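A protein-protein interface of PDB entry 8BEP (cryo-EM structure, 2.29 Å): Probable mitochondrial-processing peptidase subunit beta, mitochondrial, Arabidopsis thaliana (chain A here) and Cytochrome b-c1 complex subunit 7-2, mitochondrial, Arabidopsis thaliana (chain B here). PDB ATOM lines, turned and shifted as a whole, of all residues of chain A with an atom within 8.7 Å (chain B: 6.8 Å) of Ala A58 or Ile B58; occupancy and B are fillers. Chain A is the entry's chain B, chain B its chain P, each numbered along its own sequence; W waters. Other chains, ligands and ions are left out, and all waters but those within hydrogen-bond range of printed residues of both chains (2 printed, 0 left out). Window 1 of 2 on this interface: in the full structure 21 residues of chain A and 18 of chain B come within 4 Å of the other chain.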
ATOM      1  N   PRO A  49       7.153  25.423   2.532  1.00  0.00           N
ATOM      2  CA  PRO A  49       8.045  24.374   3.045  1.00  0.00           C
ATOM      3  C   PRO A  49       9.323  24.890   3.687  1.00  0.00           C
ATOM      4  O   PRO A  49      10.397  24.327   3.465  1.00  0.00           O
ATOM      5  CB  PRO A  49       8.358  23.552   1.791  1.00  0.00           C
ATOM      6  CG  PRO A  49       8.272  24.537   0.684  1.00  0.00           C
ATOM      7  CD  PRO A  49       7.213  25.533   1.063  1.00  0.00           C
ATOM      8  N   HIS A  50       9.225  25.953   4.481  1.00  0.00           N
ATOM      9  CA  HIS A  50      10.289  26.327   5.401  1.00  0.00           C
ATOM     10  C   HIS A  50       9.752  26.901   6.702  1.00  0.00           C
ATOM     11  O   HIS A  50      10.550  27.303   7.554  1.00  0.00           O
ATOM     12  CB  HIS A  50      11.252  27.336   4.753  1.00  0.00           C
ATOM     13  CG  HIS A  50      12.284  26.706   3.871  1.00  0.00           C
ATOM     14  ND1 HIS A  50      13.483  26.227   4.353  1.00  0.00           N
ATOM     15  CD2 HIS A  50      12.294  26.471   2.538  1.00  0.00           C
ATOM     16  CE1 HIS A  50      14.188  25.727   3.355  1.00  0.00           C
ATOM     17  NE2 HIS A  50      13.488  25.861   2.242  1.00  0.00           N
ATOM     18  N   MET A  52       7.405  25.377   9.157  1.00  0.00           N
ATOM     19  CA  MET A  52       7.508  24.406  10.232  1.00  0.00           C
ATOM     20  C   MET A  52       8.958  23.951  10.383  1.00  0.00           C
ATOM     21  O   MET A  52       9.655  23.758   9.384  1.00  0.00           O
ATOM     22  CB  MET A  52       6.602  23.206   9.964  1.00  0.00           C
ATOM     23  CG  MET A  52       5.118  23.540   9.970  1.00  0.00           C
ATOM     24  SD  MET A  52       4.678  24.806  11.176  1.00  0.00           S
ATOM     25  CE  MET A  52       4.200  23.804  12.577  1.00  0.00           C
ATOM     26  N   PRO A  53       9.442  23.790  11.616  1.00  0.00           N
ATOM     27  CA  PRO A  53      10.845  23.381  11.802  1.00  0.00           C
ATOM     28  C   PRO A  53      11.197  22.060  11.141  1.00  0.00           C
ATOM     29  O   PRO A  53      12.294  21.928  10.586  1.00  0.00           O
ATOM     30  CB  PRO A  53      10.986  23.303  13.329  1.00  0.00           C
ATOM     31  CG  PRO A  53       9.881  24.141  13.862  1.00  0.00           C
ATOM     32  CD  PRO A  53       8.753  24.023  12.895  1.00  0.00           C
ATOM     33  N   TYR A  54      10.296  21.077  11.173  1.00  0.00           N
ATOM     34  CA  TYR A  54      10.622  19.778  10.595  1.00  0.00           C
ATOM     35  C   TYR A  54      10.647  19.827   9.072  1.00  0.00           C
ATOM     36  O   TYR A  54      11.474  19.154   8.445  1.00  0.00           O
ATOM     37  CB  TYR A  54       9.643  18.713  11.095  1.00  0.00           C
ATOM     38  CG  TYR A  54       8.189  19.129  11.082  1.00  0.00           C
ATOM     39  CD1 TYR A  54       7.428  19.021   9.928  1.00  0.00           C
ATOM     40  CD2 TYR A  54       7.578  19.617  12.228  1.00  0.00           C
ATOM     41  CE1 TYR A  54       6.103  19.393   9.910  1.00  0.00           C
ATOM     42  CE2 TYR A  54       6.249  19.993  12.221  1.00  0.00           C
ATOM     43  CZ  TYR A  54       5.518  19.879  11.057  1.00  0.00           C
ATOM     44  OH  TYR A  54       4.196  20.248  11.039  1.00  0.00           O
ATOM     45  N   ASP A  55       9.768  20.624   8.462  1.00  0.00           N
ATOM     46  CA  ASP A  55       9.801  20.788   7.012  1.00  0.00           C
ATOM     47  C   ASP A  55      11.106  21.433   6.560  1.00  0.00           C
ATOM     48  O   ASP A  55      11.679  21.044   5.537  1.00  0.00           O
ATOM     49  CB  ASP A  55       8.605  21.621   6.554  1.00  0.00           C
ATOM     50  CG  ASP A  55       7.352  20.797   6.401  1.00  0.00           C
ATOM     51  OD1 ASP A  55       7.462  19.558   6.297  1.00  0.00           O
ATOM     52  OD2 ASP A  55       6.255  21.387   6.379  1.00  0.00           O
ATOM     53  N   HIS A  56      11.585  22.423   7.313  1.00  0.00           N
ATOM     54  CA  HIS A  56      12.846  23.078   6.979  1.00  0.00           C
ATOM     55  C   HIS A  56      14.016  22.101   7.049  1.00  0.00           C
ATOM     56  O   HIS A  56      14.884  22.087   6.163  1.00  0.00           O
ATOM     57  CB  HIS A  56      13.054  24.266   7.920  1.00  0.00           C
ATOM     58  CG  HIS A  56      14.419  24.867   7.849  1.00  0.00           C
ATOM     59  ND1 HIS A  56      14.855  25.597   6.765  1.00  0.00           N
ATOM     60  CD2 HIS A  56      15.443  24.856   8.734  1.00  0.00           C
ATOM     61  CE1 HIS A  56      16.092  26.005   6.982  1.00  0.00           C
ATOM     62  NE2 HIS A  56      16.471  25.571   8.170  1.00  0.00           N
ATOM     63  N   ALA A  57      14.051  21.265   8.090  1.00  0.00           N
ATOM     64  CA  ALA A  57      15.103  20.262   8.202  1.00  0.00           C
ATOM     65  C   ALA A  57      15.025  19.254   7.062  1.00  0.00           C
ATOM     66  O   ALA A  57      16.057  18.830   6.520  1.00  0.00           O
ATOM     67  CB  ALA A  57      15.009  19.561   9.555  1.00  0.00           C
ATOM     68  N   ALA A  58      13.806  18.862   6.681  1.00  0.00           N
ATOM     69  CA  ALA A  58      13.642  17.970   5.540  1.00  0.00           C
ATOM     70  C   ALA A  58      14.186  18.604   4.266  1.00  0.00           C
ATOM     71  O   ALA A  58      14.862  17.939   3.473  1.00  0.00           O
ATOM     72  CB  ALA A  58      12.172  17.596   5.377  1.00  0.00           C
ATOM     73  N   GLU A  59      13.904  19.893   4.058  1.00  0.00           N
ATOM     74  CA  GLU A  59      14.430  20.587   2.885  1.00  0.00           C
ATOM     75  C   GLU A  59      15.952  20.598   2.887  1.00  0.00           C
ATOM     76  O   GLU A  59      16.584  20.379   1.848  1.00  0.00           O
ATOM     77  CB  GLU A  59      13.893  22.016   2.827  1.00  0.00           C
ATOM     78  CG  GLU A  59      12.403  22.150   2.554  1.00  0.00           C
ATOM     79  CD  GLU A  59      11.991  21.647   1.185  1.00  0.00           C
ATOM     80  OE1 GLU A  59      11.956  20.420   0.975  1.00  0.00           O
ATOM     81  OE2 GLU A  59      11.702  22.487   0.307  1.00  0.00           O
ATOM     82  N   ILE A  60      16.559  20.856   4.048  1.00  0.00           N
ATOM     83  CA  ILE A  60      18.018  20.907   4.125  1.00  0.00           C
ATOM     84  C   ILE A  60      18.624  19.551   3.776  1.00  0.00           C
ATOM     85  O   ILE A  60      19.581  19.459   2.992  1.00  0.00           O
ATOM     86  CB  ILE A  60      18.469  21.384   5.516  1.00  0.00           C
ATOM     87  CG1 ILE A  60      18.367  22.901   5.620  1.00  0.00           C
ATOM     88  CG2 ILE A  60      19.896  20.953   5.799  1.00  0.00           C
ATOM     89  CD1 ILE A  60      18.460  23.394   7.019  1.00  0.00           C
ATOM     90  N   ILE A  61      18.078  18.478   4.353  1.00  0.00           N
ATOM     91  CA  ILE A  61      18.655  17.161   4.096  1.00  0.00           C
ATOM     92  C   ILE A  61      18.436  16.761   2.639  1.00  0.00           C
ATOM     93  O   ILE A  61      19.311  16.150   2.009  1.00  0.00           O
ATOM     94  CB  ILE A  61      18.101  16.115   5.088  1.00  0.00           C
ATOM     95  CG1 ILE A  61      18.957  14.848   5.072  1.00  0.00           C
ATOM     96  CG2 ILE A  61      16.661  15.748   4.789  1.00  0.00           C
ATOM     97  CD1 ILE A  61      20.445  15.109   5.033  1.00  0.00           C
ATOM     98  N   LYS A  62      17.286  17.133   2.067  1.00  0.00           N
ATOM     99  CA  LYS A  62      17.028  16.844   0.662  1.00  0.00           C
ATOM    100  C   LYS A  62      18.005  17.588  -0.238  1.00  0.00           C
ATOM    101  O   LYS A  62      18.468  17.045  -1.248  1.00  0.00           O
ATOM    102  CB  LYS A  62      15.583  17.205   0.316  1.00  0.00           C
ATOM    103  CG  LYS A  62      14.569  16.144   0.707  1.00  0.00           C
ATOM    104  CD  LYS A  62      13.233  16.376   0.029  1.00  0.00           C
ATOM    105  CE  LYS A  62      12.396  17.378   0.793  1.00  0.00           C
ATOM    106  NZ  LYS A  62      10.973  17.390   0.354  1.00  0.00           N
ATOM    107  N   ASN A  63      18.336  18.832   0.117  1.00  0.00           N
ATOM    108  CA  ASN A  63      19.289  19.594  -0.683  1.00  0.00           C
ATOM    109  C   ASN A  63      20.683  18.985  -0.609  1.00  0.00           C
ATOM    110  O   ASN A  63      21.388  18.906  -1.621  1.00  0.00           O
ATOM    111  CB  ASN A  63      19.314  21.052  -0.228  1.00  0.00           C
ATOM    112  CG  ASN A  63      18.086  21.815  -0.670  1.00  0.00           C
ATOM    113  OD1 ASN A  63      17.413  21.431  -1.622  1.00  0.00           O
ATOM    114  ND2 ASN A  63      17.813  22.928  -0.005  1.00  0.00           N
ATOM    115  N   LYS A  64      21.092  18.537   0.581  1.00  0.00           N
ATOM    116  CA  LYS A  64      22.376  17.848   0.705  1.00  0.00           C
ATOM    117  C   LYS A  64      22.406  16.586  -0.153  1.00  0.00           C
ATOM    118  O   LYS A  64      23.407  16.294  -0.826  1.00  0.00           O
ATOM    119  CB  LYS A  64      22.641  17.510   2.171  1.00  0.00           C
ATOM    120  CG  LYS A  64      24.106  17.472   2.557  1.00  0.00           C
ATOM    121  CD  LYS A  64      24.321  16.579   3.769  1.00  0.00           C
ATOM    122  CE  LYS A  64      25.752  16.658   4.276  1.00  0.00           C
ATOM    123  NZ  LYS A  64      26.689  17.149   3.230  1.00  0.00           N
ATOM    124  N   ILE A  65      21.310  15.830  -0.150  1.00  0.00           N
ATOM    125  CA  ILE A  65      21.255  14.602  -0.935  1.00  0.00           C
ATOM    126  C   ILE A  65      21.337  14.912  -2.426  1.00  0.00           C
ATOM    127  O   ILE A  65      22.028  14.218  -3.185  1.00  0.00           O
ATOM    128  CB  ILE A  65      19.988  13.811  -0.573  1.00  0.00           C
ATOM    129  CG1 ILE A  65      20.248  12.990   0.685  1.00  0.00           C
ATOM    130  CG2 ILE A  65      19.558  12.909  -1.720  1.00  0.00           C
ATOM    131  CD1 ILE A  65      19.219  11.962   0.951  1.00  0.00           C
ATOM    132  N   ARG B  34       0.982  12.158   5.476  1.00  0.00           N
ATOM    133  CA  ARG B  34       1.741  12.294   4.245  1.00  0.00           C
ATOM    134  C   ARG B  34       1.874  10.936   3.576  1.00  0.00           C
ATOM    135  O   ARG B  34       1.795   9.889   4.221  1.00  0.00           O
ATOM    136  CB  ARG B  34       3.125  12.877   4.514  1.00  0.00           C
ATOM    137  CG  ARG B  34       3.129  14.047   5.463  1.00  0.00           C
ATOM    138  CD  ARG B  34       3.739  15.254   4.812  1.00  0.00           C
ATOM    139  NE  ARG B  34       4.075  16.285   5.783  1.00  0.00           N
ATOM    140  CZ  ARG B  34       5.217  16.956   5.787  1.00  0.00           C
ATOM    141  NH1 ARG B  34       6.157  16.721   4.888  1.00  0.00           N
ATOM    142  NH2 ARG B  34       5.419  17.884   6.716  1.00  0.00           N
ATOM    143  N   ASP B  37       4.442   8.877   4.979  1.00  0.00           N
ATOM    144  CA  ASP B  37       4.114   8.263   6.261  1.00  0.00           C
ATOM    145  C   ASP B  37       3.602   6.838   6.109  1.00  0.00           C
ATOM    146  O   ASP B  37       3.621   6.082   7.084  1.00  0.00           O
ATOM    147  CB  ASP B  37       3.073   9.095   7.006  1.00  0.00           C
ATOM    148  CG  ASP B  37       3.575  10.467   7.374  1.00  0.00           C
ATOM    149  OD1 ASP B  37       4.802  10.645   7.485  1.00  0.00           O
ATOM    150  OD2 ASP B  37       2.734  11.368   7.552  1.00  0.00           O
ATOM    151  N   LEU B  54      17.546  10.006   8.893  1.00  0.00           N
ATOM    152  CA  LEU B  54      16.880  11.296   8.835  1.00  0.00           C
ATOM    153  C   LEU B  54      17.080  12.086  10.130  1.00  0.00           C
ATOM    154  O   LEU B  54      17.336  11.507  11.189  1.00  0.00           O
ATOM    155  CB  LEU B  54      15.390  11.116   8.564  1.00  0.00           C
ATOM    156  CG  LEU B  54      15.003  10.715   7.136  1.00  0.00           C
ATOM    157  CD1 LEU B  54      13.543  10.318   7.064  1.00  0.00           C
ATOM    158  CD2 LEU B  54      15.312  11.828   6.140  1.00  0.00           C
ATOM    159  N   PRO B  55      16.981  13.412  10.062  1.00  0.00           N
ATOM    160  CA  PRO B  55      17.060  14.227  11.282  1.00  0.00           C
ATOM    161  C   PRO B  55      15.916  13.933  12.243  1.00  0.00           C
ATOM    162  O   PRO B  55      14.821  13.539  11.839  1.00  0.00           O
ATOM    163  CB  PRO B  55      16.997  15.662  10.748  1.00  0.00           C
ATOM    164  CG  PRO B  55      17.517  15.564   9.363  1.00  0.00           C
ATOM    165  CD  PRO B  55      17.053  14.237   8.844  1.00  0.00           C
ATOM    166  N   ARG B  56      16.189  14.146  13.533  1.00  0.00           N
ATOM    167  CA  ARG B  56      15.278  13.707  14.585  1.00  0.00           C
ATOM    168  C   ARG B  56      13.925  14.409  14.509  1.00  0.00           C
ATOM    169  O   ARG B  56      12.885  13.784  14.726  1.00  0.00           O
ATOM    170  CB  ARG B  56      15.914  13.936  15.956  1.00  0.00           C
ATOM    171  CG  ARG B  56      15.045  13.486  17.111  1.00  0.00           C
ATOM    172  CD  ARG B  56      15.752  13.668  18.436  1.00  0.00           C
ATOM    173  NE  ARG B  56      14.945  13.220  19.564  1.00  0.00           N
ATOM    174  CZ  ARG B  56      15.396  13.093  20.804  1.00  0.00           C
ATOM    175  NH1 ARG B  56      16.647  13.383  21.119  1.00  0.00           N
ATOM    176  NH2 ARG B  56      14.570  12.661  21.753  1.00  0.00           N
ATOM    177  N   GLU B  57      13.919  15.712  14.227  1.00  0.00           N
ATOM    178  CA  GLU B  57      12.664  16.460  14.230  1.00  0.00           C
ATOM    179  C   GLU B  57      11.705  15.970  13.143  1.00  0.00           C
ATOM    180  O   GLU B  57      10.489  15.922  13.355  1.00  0.00           O
ATOM    181  CB  GLU B  57      12.925  17.966  14.092  1.00  0.00           C
ATOM    182  CG  GLU B  57      13.965  18.403  13.068  1.00  0.00           C
ATOM    183  CD  GLU B  57      15.397  18.074  13.471  1.00  0.00           C
ATOM    184  OE1 GLU B  57      15.642  17.821  14.671  1.00  0.00           O
ATOM    185  OE2 GLU B  57      16.280  18.087  12.590  1.00  0.00           O
ATOM    186  N   ILE B  58      12.235  15.581  11.984  1.00  0.00           N
ATOM    187  CA  ILE B  58      11.396  15.024  10.924  1.00  0.00           C
ATOM    188  C   ILE B  58      10.773  13.701  11.357  1.00  0.00           C
ATOM    189  O   ILE B  58       9.579  13.462  11.143  1.00  0.00           O
ATOM    190  CB  ILE B  58      12.204  14.874   9.624  1.00  0.00           C
ATOM    191  CG1 ILE B  58      12.930  16.180   9.318  1.00  0.00           C
ATOM    192  CG2 ILE B  58      11.325  14.409   8.479  1.00  0.00           C
ATOM    193  CD1 ILE B  58      14.133  16.012   8.481  1.00  0.00           C
ATOM    194  N   VAL B  59      11.568  12.822  11.968  1.00  0.00           N
ATOM    195  CA  VAL B  59      11.028  11.544  12.420  1.00  0.00           C
ATOM    196  C   VAL B  59      10.010  11.751  13.533  1.00  0.00           C
ATOM    197  O   VAL B  59       8.998  11.046  13.593  1.00  0.00           O
ATOM    198  CB  VAL B  59      12.168  10.603  12.851  1.00  0.00           C
ATOM    199  CG1 VAL B  59      11.617   9.247  13.262  1.00  0.00           C
ATOM    200  CG2 VAL B  59      13.163  10.446  11.726  1.00  0.00           C
ATOM    201  N   ASP B  60      10.248  12.718  14.419  1.00  0.00           N
ATOM    202  CA  ASP B  60       9.272  13.017  15.460  1.00  0.00           C
ATOM    203  C   ASP B  60       7.970  13.537  14.863  1.00  0.00           C
ATOM    204  O   ASP B  60       6.884  13.165  15.319  1.00  0.00           O
ATOM    205  CB  ASP B  60       9.849  14.020  16.457  1.00  0.00           C
ATOM    206  CG  ASP B  60      11.094  13.503  17.153  1.00  0.00           C
ATOM    207  OD1 ASP B  60      11.825  14.323  17.746  1.00  0.00           O
ATOM    208  OD2 ASP B  60      11.345  12.281  17.107  1.00  0.00           O
ATOM    209  N   ALA B  61       8.058  14.390  13.839  1.00  0.00           N
ATOM    210  CA  ALA B  61       6.852  14.863  13.163  1.00  0.00           C
ATOM    211  C   ALA B  61       6.105  13.712  12.500  1.00  0.00           C
ATOM    212  O   ALA B  61       4.871  13.645  12.560  1.00  0.00           O
ATOM    213  CB  ALA B  61       7.212  15.936  12.136  1.00  0.00           C
ATOM    214  N   ARG B  62       6.813  12.805  11.850  1.00  0.00           N
ATOM    215  CA  ARG B  62       6.222  11.584  11.260  1.00  0.00           C
ATOM    216  C   ARG B  62       5.498  10.774  12.333  1.00  0.00           C
ATOM    217  O   ARG B  62       4.337  10.428  12.094  1.00  0.00           O
ATOM    218  CB  ARG B  62       7.199  10.745  10.433  1.00  0.00           C
ATOM    219  CG  ARG B  62       6.919   9.256  10.381  1.00  0.00           C
ATOM    220  CD  ARG B  62       8.116   8.475   9.896  1.00  0.00           C
ATOM    221  NE  ARG B  62       7.838   7.055   9.877  1.00  0.00           N
ATOM    222  CZ  ARG B  62       7.446   6.352   8.826  1.00  0.00           C
ATOM    223  NH1 ARG B  62       7.296   6.923   7.646  1.00  0.00           N
ATOM    224  NH2 ARG B  62       7.226   5.062   8.958  1.00  0.00           N
ATOM    225  N   ASN B  63       6.159  10.540  13.436  1.00  0.00           N
ATOM    226  CA  ASN B  63       5.559   9.734  14.494  1.00  0.00           C
ATOM    227  C   ASN B  63       4.329  10.414  15.082  1.00  0.00           C
ATOM    228  O   ASN B  63       3.336   9.748  15.394  1.00  0.00           O
ATOM    229  CB  ASN B  63       6.589   9.443  15.588  1.00  0.00           C
ATOM    230  CG  ASN B  63       7.667   8.478  15.135  1.00  0.00           C
ATOM    231  OD1 ASN B  63       7.416   7.575  14.341  1.00  0.00           O
ATOM    232  ND2 ASN B  63       8.878   8.671  15.635  1.00  0.00           N
ATOM    233  N   ARG B  65       2.333  12.513  13.485  1.00  0.00           N
ATOM    234  CA  ARG B  65       1.273  12.370  12.494  1.00  0.00           C
ATOM    235  C   ARG B  65       0.698  10.959  12.514  1.00  0.00           C
ATOM    236  O   ARG B  65      -0.514  10.772  12.379  1.00  0.00           O
ATOM    237  CB  ARG B  65       1.795  12.723  11.099  1.00  0.00           C
ATOM    238  CG  ARG B  65       1.977  14.209  10.860  1.00  0.00           C
ATOM    239  CD  ARG B  65       2.242  14.521   9.392  1.00  0.00           C
ATOM    240  NE  ARG B  65       3.389  13.791   8.865  1.00  0.00           N
ATOM    241  CZ  ARG B  65       4.629  14.258   8.836  1.00  0.00           C
ATOM    242  NH1 ARG B  65       4.922  15.471   9.271  1.00  0.00           N
ATOM    243  NH2 ARG B  65       5.601  13.485   8.365  1.00  0.00           N
ATOM    244  N   ARG B  91       4.043  16.414   0.346  1.00  0.00           N
ATOM    245  CA  ARG B  91       5.337  16.990   0.682  1.00  0.00           C
ATOM    246  C   ARG B  91       6.241  15.876   1.198  1.00  0.00           C
ATOM    247  O   ARG B  91       5.924  15.229   2.200  1.00  0.00           O
ATOM    248  CB  ARG B  91       5.176  18.095   1.719  1.00  0.00           C
ATOM    249  CG  ARG B  91       6.461  18.815   2.072  1.00  0.00           C
ATOM    250  CD  ARG B  91       6.182  20.009   2.952  1.00  0.00           C
ATOM    251  NE  ARG B  91       5.359  21.002   2.273  1.00  0.00           N
ATOM    252  CZ  ARG B  91       4.960  22.143   2.816  1.00  0.00           C
ATOM    253  NH1 ARG B  91       5.289  22.471   4.053  1.00  0.00           N
ATOM    254  NH2 ARG B  91       4.210  22.974   2.099  1.00  0.00           N
ATOM    255  N   SER B  92       7.356  15.646   0.513  1.00  0.00           N
ATOM    256  CA  SER B  92       8.181  14.476   0.768  1.00  0.00           C
ATOM    257  C   SER B  92       9.268  14.756   1.799  1.00  0.00           C
ATOM    258  O   SER B  92       9.771  15.875   1.924  1.00  0.00           O
ATOM    259  CB  SER B  92       8.823  13.978  -0.528  1.00  0.00           C
ATOM    260  OG  SER B  92       9.277  12.638  -0.396  1.00  0.00           O
ATOM    261  N   TYR B  93       9.616  13.713   2.550  1.00  0.00           N
ATOM    262  CA  TYR B  93      10.778  13.734   3.427  1.00  0.00           C
ATOM    263  C   TYR B  93      11.610  12.465   3.350  1.00  0.00           C
ATOM    264  O   TYR B  93      12.683  12.425   3.954  1.00  0.00           O
ATOM    265  CB  TYR B  93      10.350  13.964   4.887  1.00  0.00           C
ATOM    266  CG  TYR B  93       9.454  12.882   5.447  1.00  0.00           C
ATOM    267  CD1 TYR B  93       9.987  11.705   5.964  1.00  0.00           C
ATOM    268  CD2 TYR B  93       8.076  13.032   5.453  1.00  0.00           C
ATOM    269  CE1 TYR B  93       9.174  10.714   6.467  1.00  0.00           C
ATOM    270  CE2 TYR B  93       7.253  12.046   5.957  1.00  0.00           C
ATOM    271  CZ  TYR B  93       7.809  10.888   6.465  1.00  0.00           C
ATOM    272  OH  TYR B  93       6.996   9.904   6.970  1.00  0.00           O
ATOM    273  N   LEU B  94      11.161  11.434   2.638  1.00  0.00           N
ATOM    274  CA  LEU B  94      11.770  10.116   2.701  1.00  0.00           C
ATOM    275  C   LEU B  94      12.326   9.615   1.377  1.00  0.00           C
ATOM    276  O   LEU B  94      13.313   8.877   1.385  1.00  0.00           O
ATOM    277  CB  LEU B  94      10.749   9.090   3.219  1.00  0.00           C
ATOM    278  CG  LEU B  94      11.251   7.662   3.423  1.00  0.00           C
ATOM    279  CD1 LEU B  94      12.337   7.615   4.491  1.00  0.00           C
ATOM    280  CD2 LEU B  94      10.104   6.750   3.784  1.00  0.00           C
HETATM  281  O   HOH W   1       5.892  24.246   6.397  1.00  0.00           O
HETATM  282  O   HOH W   2       8.710  17.554   4.658  1.00  0.00           O
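Of the 17 printed residues of chain B, 6 touch a printed residue of chain A.
Of the 16 printed residues of chain A, 6 touch a printed residue of chain B.
NZ of Lys A62 lies within salt-bridge range of OE1 of Glu A59, at 3.2 Å.
N of Arg B34 lies within hydrogen-bond range of OD2 of Asp B37 (2.8 Å).
The backbone carbonyl oxygen (O) of Arg B91 is in hydrogen-bond range of the guanidinium group (NH1) of Arg B34 (3.1 Å).
Pro A49 touches Arg B91 (CA to NH1, 3.5 Å).
Arg B34 touches Tyr A54 (NH2 to CE1, 3.6 Å).
Tyr A54 touches Glu B57.
Tyr A54 touches Ile B58.
Tyr A54 touches Ala B61.
CB of Ala A57 touches OE2 of Glu B57 (3.6 Å).
Ala A57 touches Ile B58.
Ile B58 touches Ala A58.
Water W2 lies within hydrogen-bond range of NH1 of Arg B34 (2.7 Å), OD1 of Asp A55 (2.9 Å) and O of Ser B92 (3.4 Å).
Water W1 lies within hydrogen-bond range of OD2 of Asp A55 (2.9 Å), NH1 of Arg B91 (3.0 Å) and N of Met A52 (3.3 Å).
Of the printed residues of chain B, Asp A55 touches Arg B34 (2.7 Å) and Arg B91 (2.7 Å).
Of the printed residues of chain B, Ala A58 touches Ile B58 (3.4 Å).
Of the printed residues of chain B, Lys A62 touches Ser B92.
Ile A65 touches none of the printed residues of chain B.
No residue of chain A comes within 4 Å of Pro B55.
Ile B58 touches just these residues of chain A: Tyr A54, Ala A57 and Ala A58.
Arg B62 touches none of the printed residues of chain A.
Printed residues of chain A within 4 Å of Arg B91: Pro A49 and Asp A55.
The guanidinium group of Arg B34 is in salt-bridge range of the side-chain carboxylate of Asp A55.
The side-chain carboxylate (OD2) of Asp A55 lies within salt-bridge range of the guanidinium group (NH1) of Arg B91.
The side-chain amino group (NZ) of Lys A62 is in hydrogen-bond range of the backbone carbonyl oxygen (O) of Ser B92 (2.5 Å).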
